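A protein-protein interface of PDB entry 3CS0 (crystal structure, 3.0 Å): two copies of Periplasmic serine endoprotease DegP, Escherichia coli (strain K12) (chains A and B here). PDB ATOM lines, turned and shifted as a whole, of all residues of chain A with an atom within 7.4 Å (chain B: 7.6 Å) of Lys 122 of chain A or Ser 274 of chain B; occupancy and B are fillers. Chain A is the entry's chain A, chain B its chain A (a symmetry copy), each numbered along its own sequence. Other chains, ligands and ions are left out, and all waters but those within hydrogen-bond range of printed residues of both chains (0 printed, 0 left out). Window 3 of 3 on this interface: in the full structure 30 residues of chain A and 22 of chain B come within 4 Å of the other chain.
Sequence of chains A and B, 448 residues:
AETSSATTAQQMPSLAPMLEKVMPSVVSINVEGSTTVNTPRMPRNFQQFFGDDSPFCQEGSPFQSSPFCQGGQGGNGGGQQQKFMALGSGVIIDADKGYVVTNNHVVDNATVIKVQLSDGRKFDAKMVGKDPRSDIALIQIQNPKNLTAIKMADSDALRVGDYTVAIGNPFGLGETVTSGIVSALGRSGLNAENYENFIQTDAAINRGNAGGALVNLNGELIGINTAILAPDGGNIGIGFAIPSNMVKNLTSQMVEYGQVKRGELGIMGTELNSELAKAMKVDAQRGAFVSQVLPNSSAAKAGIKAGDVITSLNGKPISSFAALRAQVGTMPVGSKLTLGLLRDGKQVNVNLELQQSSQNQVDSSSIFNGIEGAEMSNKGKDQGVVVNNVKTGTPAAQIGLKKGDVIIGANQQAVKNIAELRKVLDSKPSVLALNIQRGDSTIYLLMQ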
ATOM      1  N   ASN A  30      -4.152 -20.454   6.375  1.00  0.00           N
ATOM      2  CA  ASN A  30      -4.439 -21.168   7.616  1.00  0.00           C
ATOM      3  C   ASN A  30      -5.892 -20.947   7.955  1.00  0.00           C
ATOM      4  O   ASN A  30      -6.376 -19.818   7.958  1.00  0.00           O
ATOM      5  CB  ASN A  30      -3.532 -20.681   8.728  1.00  0.00           C
ATOM      6  CG  ASN A  30      -2.107 -21.122   8.514  1.00  0.00           C
ATOM      7  OD1 ASN A  30      -1.810 -22.315   8.594  1.00  0.00           O
ATOM      8  ND2 ASN A  30      -1.217 -20.170   8.208  1.00  0.00           N
ATOM      9  N   LYS A 114      -6.564 -17.038   7.818  1.00  0.00           N
ATOM     10  CA  LYS A 114      -5.409 -16.143   7.804  1.00  0.00           C
ATOM     11  C   LYS A 114      -4.419 -16.498   6.671  1.00  0.00           C
ATOM     12  O   LYS A 114      -4.043 -17.659   6.491  1.00  0.00           O
ATOM     13  CB  LYS A 114      -4.723 -16.136   9.186  1.00  0.00           C
ATOM     14  CG  LYS A 114      -5.582 -15.435  10.271  1.00  0.00           C
ATOM     15  CD  LYS A 114      -4.849 -15.204  11.605  1.00  0.00           C
ATOM     16  CE  LYS A 114      -4.718 -13.701  11.949  1.00  0.00           C
ATOM     17  NZ  LYS A 114      -3.569 -13.386  12.908  1.00  0.00           N
ATOM     18  N   VAL A 115      -4.034 -15.474   5.909  1.00  0.00           N
ATOM     19  CA  VAL A 115      -3.123 -15.579   4.776  1.00  0.00           C
ATOM     20  C   VAL A 115      -1.703 -15.154   5.148  1.00  0.00           C
ATOM     21  O   VAL A 115      -1.523 -14.112   5.776  1.00  0.00           O
ATOM     22  CB  VAL A 115      -3.604 -14.653   3.641  1.00  0.00           C
ATOM     23  CG1 VAL A 115      -2.458 -14.350   2.669  1.00  0.00           C
ATOM     24  CG2 VAL A 115      -4.788 -15.286   2.926  1.00  0.00           C
ATOM     25  N   GLN A 116      -0.691 -15.934   4.767  1.00  0.00           N
ATOM     26  CA  GLN A 116       0.685 -15.540   5.078  1.00  0.00           C
ATOM     27  C   GLN A 116       1.576 -15.455   3.839  1.00  0.00           C
ATOM     28  O   GLN A 116       1.787 -16.455   3.137  1.00  0.00           O
ATOM     29  CB  GLN A 116       1.330 -16.488   6.077  1.00  0.00           C
ATOM     30  CG  GLN A 116       2.730 -16.006   6.436  1.00  0.00           C
ATOM     31  CD  GLN A 116       3.487 -16.940   7.355  1.00  0.00           C
ATOM     32  OE1 GLN A 116       4.679 -16.745   7.581  1.00  0.00           O
ATOM     33  NE2 GLN A 116       2.804 -17.952   7.896  1.00  0.00           N
ATOM     34  N   LEU A 117       2.114 -14.263   3.584  1.00  0.00           N
ATOM     35  CA  LEU A 117       2.960 -14.051   2.418  1.00  0.00           C
ATOM     36  C   LEU A 117       4.299 -14.758   2.499  1.00  0.00           C
ATOM     37  O   LEU A 117       4.678 -15.281   3.553  1.00  0.00           O
ATOM     38  CB  LEU A 117       3.193 -12.559   2.196  1.00  0.00           C
ATOM     39  CG  LEU A 117       1.895 -11.775   2.185  1.00  0.00           C
ATOM     40  CD1 LEU A 117       2.140 -10.404   1.607  1.00  0.00           C
ATOM     41  CD2 LEU A 117       0.877 -12.512   1.362  1.00  0.00           C
ATOM     42  N   ASP A 119       7.103 -13.344   2.392  1.00  0.00           N
ATOM     43  CA  ASP A 119       8.033 -12.506   3.162  1.00  0.00           C
ATOM     44  C   ASP A 119       7.832 -12.575   4.668  1.00  0.00           C
ATOM     45  O   ASP A 119       8.604 -11.981   5.421  1.00  0.00           O
ATOM     46  CB  ASP A 119       7.952 -11.035   2.733  1.00  0.00           C
ATOM     47  CG  ASP A 119       6.639 -10.362   3.138  1.00  0.00           C
ATOM     48  OD1 ASP A 119       5.924 -10.899   4.031  1.00  0.00           O
ATOM     49  OD2 ASP A 119       6.343  -9.278   2.564  1.00  0.00           O
ATOM     50  N   GLY A 120       6.791 -13.278   5.103  1.00  0.00           N
ATOM     51  CA  GLY A 120       6.543 -13.411   6.522  1.00  0.00           C
ATOM     52  C   GLY A 120       5.244 -12.792   6.984  1.00  0.00           C
ATOM     53  O   GLY A 120       4.541 -13.356   7.838  1.00  0.00           O
ATOM     54  N   ARG A 121       4.914 -11.638   6.415  1.00  0.00           N
ATOM     55  CA  ARG A 121       3.702 -10.921   6.787  1.00  0.00           C
ATOM     56  C   ARG A 121       2.440 -11.775   6.847  1.00  0.00           C
ATOM     57  O   ARG A 121       2.201 -12.605   5.962  1.00  0.00           O
ATOM     58  CB  ARG A 121       3.462  -9.764   5.816  1.00  0.00           C
ATOM     59  CG  ARG A 121       4.434  -8.622   5.968  1.00  0.00           C
ATOM     60  CD  ARG A 121       4.043  -7.486   5.064  1.00  0.00           C
ATOM     61  NE  ARG A 121       4.379  -7.778   3.677  1.00  0.00           N
ATOM     62  CZ  ARG A 121       3.673  -7.357   2.632  1.00  0.00           C
ATOM     63  NH1 ARG A 121       2.581  -6.624   2.818  1.00  0.00           N
ATOM     64  NH2 ARG A 121       4.060  -7.672   1.403  1.00  0.00           N
ATOM     65  N   LYS A 122       1.637 -11.568   7.893  1.00  0.00           N
ATOM     66  CA  LYS A 122       0.361 -12.274   8.039  1.00  0.00           C
ATOM     67  C   LYS A 122      -0.781 -11.282   7.941  1.00  0.00           C
ATOM     68  O   LYS A 122      -0.660 -10.167   8.421  1.00  0.00           O
ATOM     69  CB  LYS A 122       0.256 -12.984   9.380  1.00  0.00           C
ATOM     70  CG  LYS A 122       1.166 -14.162   9.513  1.00  0.00           C
ATOM     71  CD  LYS A 122       0.501 -15.265  10.315  1.00  0.00           C
ATOM     72  CE  LYS A 122       1.383 -16.501  10.328  1.00  0.00           C
ATOM     73  NZ  LYS A 122       2.762 -16.165  10.825  1.00  0.00           N
ATOM     74  N   PHE A 123      -1.873 -11.678   7.298  1.00  0.00           N
ATOM     75  CA  PHE A 123      -3.056 -10.829   7.165  1.00  0.00           C
ATOM     76  C   PHE A 123      -4.284 -11.688   7.420  1.00  0.00           C
ATOM     77  O   PHE A 123      -4.213 -12.928   7.435  1.00  0.00           O
ATOM     78  CB  PHE A 123      -3.212 -10.267   5.759  1.00  0.00           C
ATOM     79  CG  PHE A 123      -2.081  -9.427   5.299  1.00  0.00           C
ATOM     80  CD1 PHE A 123      -0.850  -9.992   5.019  1.00  0.00           C
ATOM     81  CD2 PHE A 123      -2.276  -8.082   5.034  1.00  0.00           C
ATOM     82  CE1 PHE A 123       0.176  -9.227   4.469  1.00  0.00           C
ATOM     83  CE2 PHE A 123      -1.265  -7.307   4.483  1.00  0.00           C
ATOM     84  CZ  PHE A 123      -0.038  -7.879   4.198  1.00  0.00           C
ATOM     85  N   ASP A 124      -5.423 -11.039   7.618  1.00  0.00           N
ATOM     86  CA  ASP A 124      -6.642 -11.808   7.802  1.00  0.00           C
ATOM     87  C   ASP A 124      -7.400 -11.649   6.504  1.00  0.00           C
ATOM     88  O   ASP A 124      -7.336 -10.602   5.843  1.00  0.00           O
ATOM     89  CB  ASP A 124      -7.453 -11.292   9.003  1.00  0.00           C
ATOM     90  CG  ASP A 124      -6.891 -11.790  10.341  1.00  0.00           C
ATOM     91  OD1 ASP A 124      -7.353 -12.849  10.826  1.00  0.00           O
ATOM     92  OD2 ASP A 124      -5.971 -11.138  10.901  1.00  0.00           O
ATOM     93  N   ILE A 141      -7.937 -10.597   1.152  1.00  0.00           N
ATOM     94  CA  ILE A 141      -7.052 -10.149   2.218  1.00  0.00           C
ATOM     95  C   ILE A 141      -7.572  -8.804   2.728  1.00  0.00           C
ATOM     96  O   ILE A 141      -7.757  -7.860   1.952  1.00  0.00           O
ATOM     97  CB  ILE A 141      -5.582  -9.976   1.676  1.00  0.00           C
ATOM     98  CG1 ILE A 141      -5.015 -11.331   1.242  1.00  0.00           C
ATOM     99  CG2 ILE A 141      -4.694  -9.353   2.740  1.00  0.00           C
ATOM    100  CD1 ILE A 141      -3.695 -11.258   0.489  1.00  0.00           C
ATOM    101  N   GLN A 142      -7.822  -8.722   4.031  1.00  0.00           N
ATOM    102  CA  GLN A 142      -8.316  -7.484   4.631  1.00  0.00           C
ATOM    103  C   GLN A 142      -7.142  -6.533   4.850  1.00  0.00           C
ATOM    104  O   GLN A 142      -6.198  -6.865   5.558  1.00  0.00           O
ATOM    105  CB  GLN A 142      -8.982  -7.780   5.975  1.00  0.00           C
ATOM    106  CG  GLN A 142     -10.166  -8.741   5.935  1.00  0.00           C
ATOM    107  CD  GLN A 142     -11.356  -8.205   5.141  1.00  0.00           C
ATOM    108  OE1 GLN A 142     -11.421  -8.366   3.914  1.00  0.00           O
ATOM    109  NE2 GLN A 142     -12.300  -7.560   5.837  1.00  0.00           N
ATOM    110  N   GLU B 271      12.630 -17.285  17.073  1.00  0.00           N
ATOM    111  CA  GLU B 271      12.223 -16.871  15.752  1.00  0.00           C
ATOM    112  C   GLU B 271      11.393 -15.588  15.850  1.00  0.00           C
ATOM    113  O   GLU B 271      10.469 -15.491  16.669  1.00  0.00           O
ATOM    114  CB  GLU B 271      11.411 -17.988  15.107  1.00  0.00           C
ATOM    115  CG  GLU B 271      12.085 -19.348  15.159  1.00  0.00           C
ATOM    116  CD  GLU B 271      13.366 -19.408  14.344  1.00  0.00           C
ATOM    117  OE1 GLU B 271      13.641 -18.444  13.593  1.00  0.00           O
ATOM    118  OE2 GLU B 271      14.094 -20.425  14.453  1.00  0.00           O
ATOM    119  N   LEU B 272      11.735 -14.604  15.023  1.00  0.00           N
ATOM    120  CA  LEU B 272      11.020 -13.341  15.011  1.00  0.00           C
ATOM    121  C   LEU B 272       9.853 -13.378  14.036  1.00  0.00           C
ATOM    122  O   LEU B 272      10.002 -12.943  12.898  1.00  0.00           O
ATOM    123  CB  LEU B 272      11.979 -12.207  14.622  1.00  0.00           C
ATOM    124  CG  LEU B 272      11.467 -10.763  14.456  1.00  0.00           C
ATOM    125  CD1 LEU B 272      11.096 -10.497  13.032  1.00  0.00           C
ATOM    126  CD2 LEU B 272      10.284 -10.504  15.387  1.00  0.00           C
ATOM    127  N   ASN B 273       8.699 -13.888  14.471  1.00  0.00           N
ATOM    128  CA  ASN B 273       7.515 -13.952  13.602  1.00  0.00           C
ATOM    129  C   ASN B 273       6.814 -12.584  13.438  1.00  0.00           C
ATOM    130  O   ASN B 273       7.232 -11.594  14.033  1.00  0.00           O
ATOM    131  CB  ASN B 273       6.521 -15.008  14.109  1.00  0.00           C
ATOM    132  CG  ASN B 273       5.883 -14.643  15.438  1.00  0.00           C
ATOM    133  OD1 ASN B 273       6.509 -14.727  16.496  1.00  0.00           O
ATOM    134  ND2 ASN B 273       4.619 -14.243  15.390  1.00  0.00           N
ATOM    135  N   SER B 274       5.763 -12.521  12.622  1.00  0.00           N
ATOM    136  CA  SER B 274       5.062 -11.260  12.387  1.00  0.00           C
ATOM    137  C   SER B 274       4.374 -10.728  13.638  1.00  0.00           C
ATOM    138  O   SER B 274       4.348  -9.520  13.879  1.00  0.00           O
ATOM    139  CB  SER B 274       4.025 -11.425  11.272  1.00  0.00           C
ATOM    140  OG  SER B 274       3.660 -10.167  10.718  1.00  0.00           O
ATOM    141  N   GLU B 275       3.817 -11.626  14.436  1.00  0.00           N
ATOM    142  CA  GLU B 275       3.138 -11.216  15.658  1.00  0.00           C
ATOM    143  C   GLU B 275       4.116 -10.555  16.629  1.00  0.00           C
ATOM    144  O   GLU B 275       3.914  -9.406  17.025  1.00  0.00           O
ATOM    145  CB  GLU B 275       2.461 -12.421  16.317  1.00  0.00           C
ATOM    146  CG  GLU B 275       1.612 -13.254  15.349  1.00  0.00           C
ATOM    147  CD  GLU B 275       0.586 -12.420  14.580  1.00  0.00           C
ATOM    148  OE1 GLU B 275       0.989 -11.457  13.883  1.00  0.00           O
ATOM    149  OE2 GLU B 275      -0.626 -12.735  14.666  1.00  0.00           O
ATOM    150  N   LEU B 276       5.177 -11.266  17.006  1.00  0.00           N
ATOM    151  CA  LEU B 276       6.164 -10.703  17.922  1.00  0.00           C
ATOM    152  C   LEU B 276       6.741  -9.378  17.395  1.00  0.00           C
ATOM    153  O   LEU B 276       7.127  -8.499  18.167  1.00  0.00           O
ATOM    154  CB  LEU B 276       7.302 -11.701  18.161  1.00  0.00           C
ATOM    155  CG  LEU B 276       8.559 -11.145  18.859  1.00  0.00           C
ATOM    156  CD1 LEU B 276       8.191 -10.568  20.213  1.00  0.00           C
ATOM    157  CD2 LEU B 276       9.608 -12.232  19.016  1.00  0.00           C
ATOM    158  N   ALA B 277       6.789  -9.228  16.081  1.00  0.00           N
ATOM    159  CA  ALA B 277       7.334  -8.018  15.497  1.00  0.00           C
ATOM    160  C   ALA B 277       6.426  -6.809  15.710  1.00  0.00           C
ATOM    161  O   ALA B 277       6.905  -5.670  15.743  1.00  0.00           O
ATOM    162  CB  ALA B 277       7.594  -8.234  14.007  1.00  0.00           C
ATOM    163  N   LYS B 278       5.122  -7.047  15.842  1.00  0.00           N
ATOM    164  CA  LYS B 278       4.175  -5.953  16.067  1.00  0.00           C
ATOM    165  C   LYS B 278       4.371  -5.530  17.510  1.00  0.00           C
ATOM    166  O   LYS B 278       4.686  -4.371  17.800  1.00  0.00           O
ATOM    167  CB  LYS B 278       2.728  -6.422  15.871  1.00  0.00           C
ATOM    168  CG  LYS B 278       2.473  -7.139  14.546  1.00  0.00           C
ATOM    169  CD  LYS B 278       1.063  -7.738  14.471  1.00  0.00           C
ATOM    170  CE  LYS B 278       0.003  -6.660  14.308  1.00  0.00           C
ATOM    171  NZ  LYS B 278       0.187  -5.889  13.031  1.00  0.00           N
ATOM    172  N   ALA B 279       4.195  -6.496  18.411  1.00  0.00           N
ATOM    173  CA  ALA B 279       4.360  -6.263  19.840  1.00  0.00           C
ATOM    174  C   ALA B 279       5.653  -5.493  20.093  1.00  0.00           C
ATOM    175  O   ALA B 279       5.702  -4.618  20.947  1.00  0.00           O
ATOM    176  CB  ALA B 279       4.385  -7.602  20.588  1.00  0.00           C
ATOM    177  N   MET B 280       6.693  -5.803  19.326  1.00  0.00           N
ATOM    178  CA  MET B 280       7.989  -5.157  19.491  1.00  0.00           C
ATOM    179  C   MET B 280       8.280  -3.994  18.523  1.00  0.00           C
ATOM    180  O   MET B 280       9.400  -3.482  18.486  1.00  0.00           O
ATOM    181  CB  MET B 280       9.091  -6.214  19.365  1.00  0.00           C
ATOM    182  CG  MET B 280      10.287  -5.994  20.272  1.00  0.00           C
ATOM    183  SD  MET B 280       9.886  -6.378  22.124  1.00  0.00           S
ATOM    184  CE  MET B 280       8.992  -4.743  22.587  1.00  0.00           C
ATOM    185  N   VAL B 282       8.842  -3.715  15.208  1.00  0.00           N
ATOM    186  CA  VAL B 282       9.988  -3.837  14.311  1.00  0.00           C
ATOM    187  C   VAL B 282       9.526  -4.179  12.903  1.00  0.00           C
ATOM    188  O   VAL B 282       8.714  -5.090  12.702  1.00  0.00           O
ATOM    189  CB  VAL B 282      11.015  -4.898  14.788  1.00  0.00           C
ATOM    190  CG1 VAL B 282      11.342  -4.667  16.249  1.00  0.00           C
ATOM    191  CG2 VAL B 282      10.491  -6.308  14.556  1.00  0.00           C
ATOM    192  N   ALA B 284      10.047  -5.987  10.234  1.00  0.00           N
ATOM    193  CA  ALA B 284      10.760  -7.182   9.828  1.00  0.00           C
ATOM    194  C   ALA B 284       9.910  -8.353  10.258  1.00  0.00           C
ATOM    195  O   ALA B 284       9.520  -8.444  11.425  1.00  0.00           O
ATOM    196  CB  ALA B 284      12.109  -7.240  10.517  1.00  0.00           C
ATOM    197  N   GLN B 285       9.613  -9.246   9.322  1.00  0.00           N
ATOM    198  CA  GLN B 285       8.792 -10.404   9.636  1.00  0.00           C
ATOM    199  C   GLN B 285       9.626 -11.664   9.825  1.00  0.00           C
ATOM    200  O   GLN B 285       9.096 -12.749  10.062  1.00  0.00           O
ATOM    201  CB  GLN B 285       7.754 -10.609   8.533  1.00  0.00           C
ATOM    202  CG  GLN B 285       6.368 -10.038   8.849  1.00  0.00           C
ATOM    203  CD  GLN B 285       6.388  -8.560   9.208  1.00  0.00           C
ATOM    204  OE1 GLN B 285       7.050  -7.752   8.543  1.00  0.00           O
ATOM    205  NE2 GLN B 285       5.646  -8.197  10.263  1.00  0.00           N
ATOM    206  N   ARG B 286      10.941 -11.508   9.731  1.00  0.00           N
ATOM    207  CA  ARG B 286      11.850 -12.632   9.888  1.00  0.00           C
ATOM    208  C   ARG B 286      13.199 -12.192  10.426  1.00  0.00           C
ATOM    209  O   ARG B 286      13.673 -11.089  10.124  1.00  0.00           O
ATOM    210  CB  ARG B 286      12.034 -13.329   8.545  1.00  0.00           C
ATOM    211  CG  ARG B 286      11.596 -14.779   8.565  1.00  0.00           C
ATOM    212  CD  ARG B 286      10.647 -15.060   7.427  1.00  0.00           C
ATOM    213  NE  ARG B 286      11.191 -14.558   6.174  1.00  0.00           N
ATOM    214  CZ  ARG B 286      10.594 -14.708   5.002  1.00  0.00           C
ATOM    215  NH1 ARG B 286       9.432 -15.349   4.936  1.00  0.00           N
ATOM    216  NH2 ARG B 286      11.153 -14.214   3.902  1.00  0.00           N
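The backbone NH (N) of Gly 120 of chain A lies close to the guanidinium group (NH1) of Arg 286 of chain B (3.4 Å). The side-chain amino group of Lys 114 of chain A lies within salt-bridge range of the side-chain carboxylate of Glu 275 of chain B.
O of Asn 30 of chain A lies within hydrogen-bond range of N of Lys 114 of chain A, at 2.8 Å. The side-chain hydroxyl of Ser 274 of chain B is in hydrogen-bond range of the side-chain amide nitrogen of Gln 285 of chain B (2.8 Å). ND2 of Asn 273 of chain B lies close to N of Glu 275 of chain B (2.9 Å). NE2 of Gln 116 of chain A lies close to NZ of Lys 122 of chain A (3.4 Å). OD2 of Asp 119 of chain A is in salt-bridge range of NE of Arg 121 of chain A (2.7 Å). The side-chain carboxylate (OD2) of Asp 124 of chain A lies within salt-bridge range of the side-chain amino group (NZ) of Lys 114 of chain A, 3.9 Å away.
Among the printed residues, merely in contact across the chains: Asp 119 of chain A with Arg 286 of chain B (3.2 Å), Arg 121 of chain A with Gln 285 of chain B (3.3 Å), Asp 119 of chain A with Gln 285 of chain B (3.5 Å), Gly 120 of chain A with Gln 285 of chain B (3.5 Å), Lys 122 of chain A with Ser 274 of chain B (3.7 Å) and Gly 120 of chain A with Ser 274 of chain B (3.97 Å).
Printed residues of chain B within 4 Å of Lys 114 of chain A: Glu 275. Of the printed residues of chain B, Gly 120 of chain A touches Ser 274, Gln 285 and Arg 286. Printed residues of chain B within 4 Å of Arg 121 of chain A: Gln 285 (3.3 Å). Lys 122 of chain A touches just one residue of chain B: Ser 274. Of the printed residues of chain A, Ser 274 of chain B touches Gly 120 and Lys 122. Of the printed residues of chain A, Glu 275 of chain B touches Lys 114 (3.5 Å). Of the printed residues of chain A, Gln 285 of chain B touches Asp 119 (3.5 Å), Gly 120 (3.5 Å) and Arg 121 (3.3 Å). The nearest printed residue of chain A that does not touch Ser 274 of chain B is Arg 121 of chain A (4.003 Å).
Of the 14 printed residues of chain B, 4 touch a printed residue of chain A. Among the printed residues, 8 pairs touch across the chains.
No position is printed for both chains. Of the 8 pairs that touch across the chains among the printed residues, none has its exchanged pair printed and touching as well.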
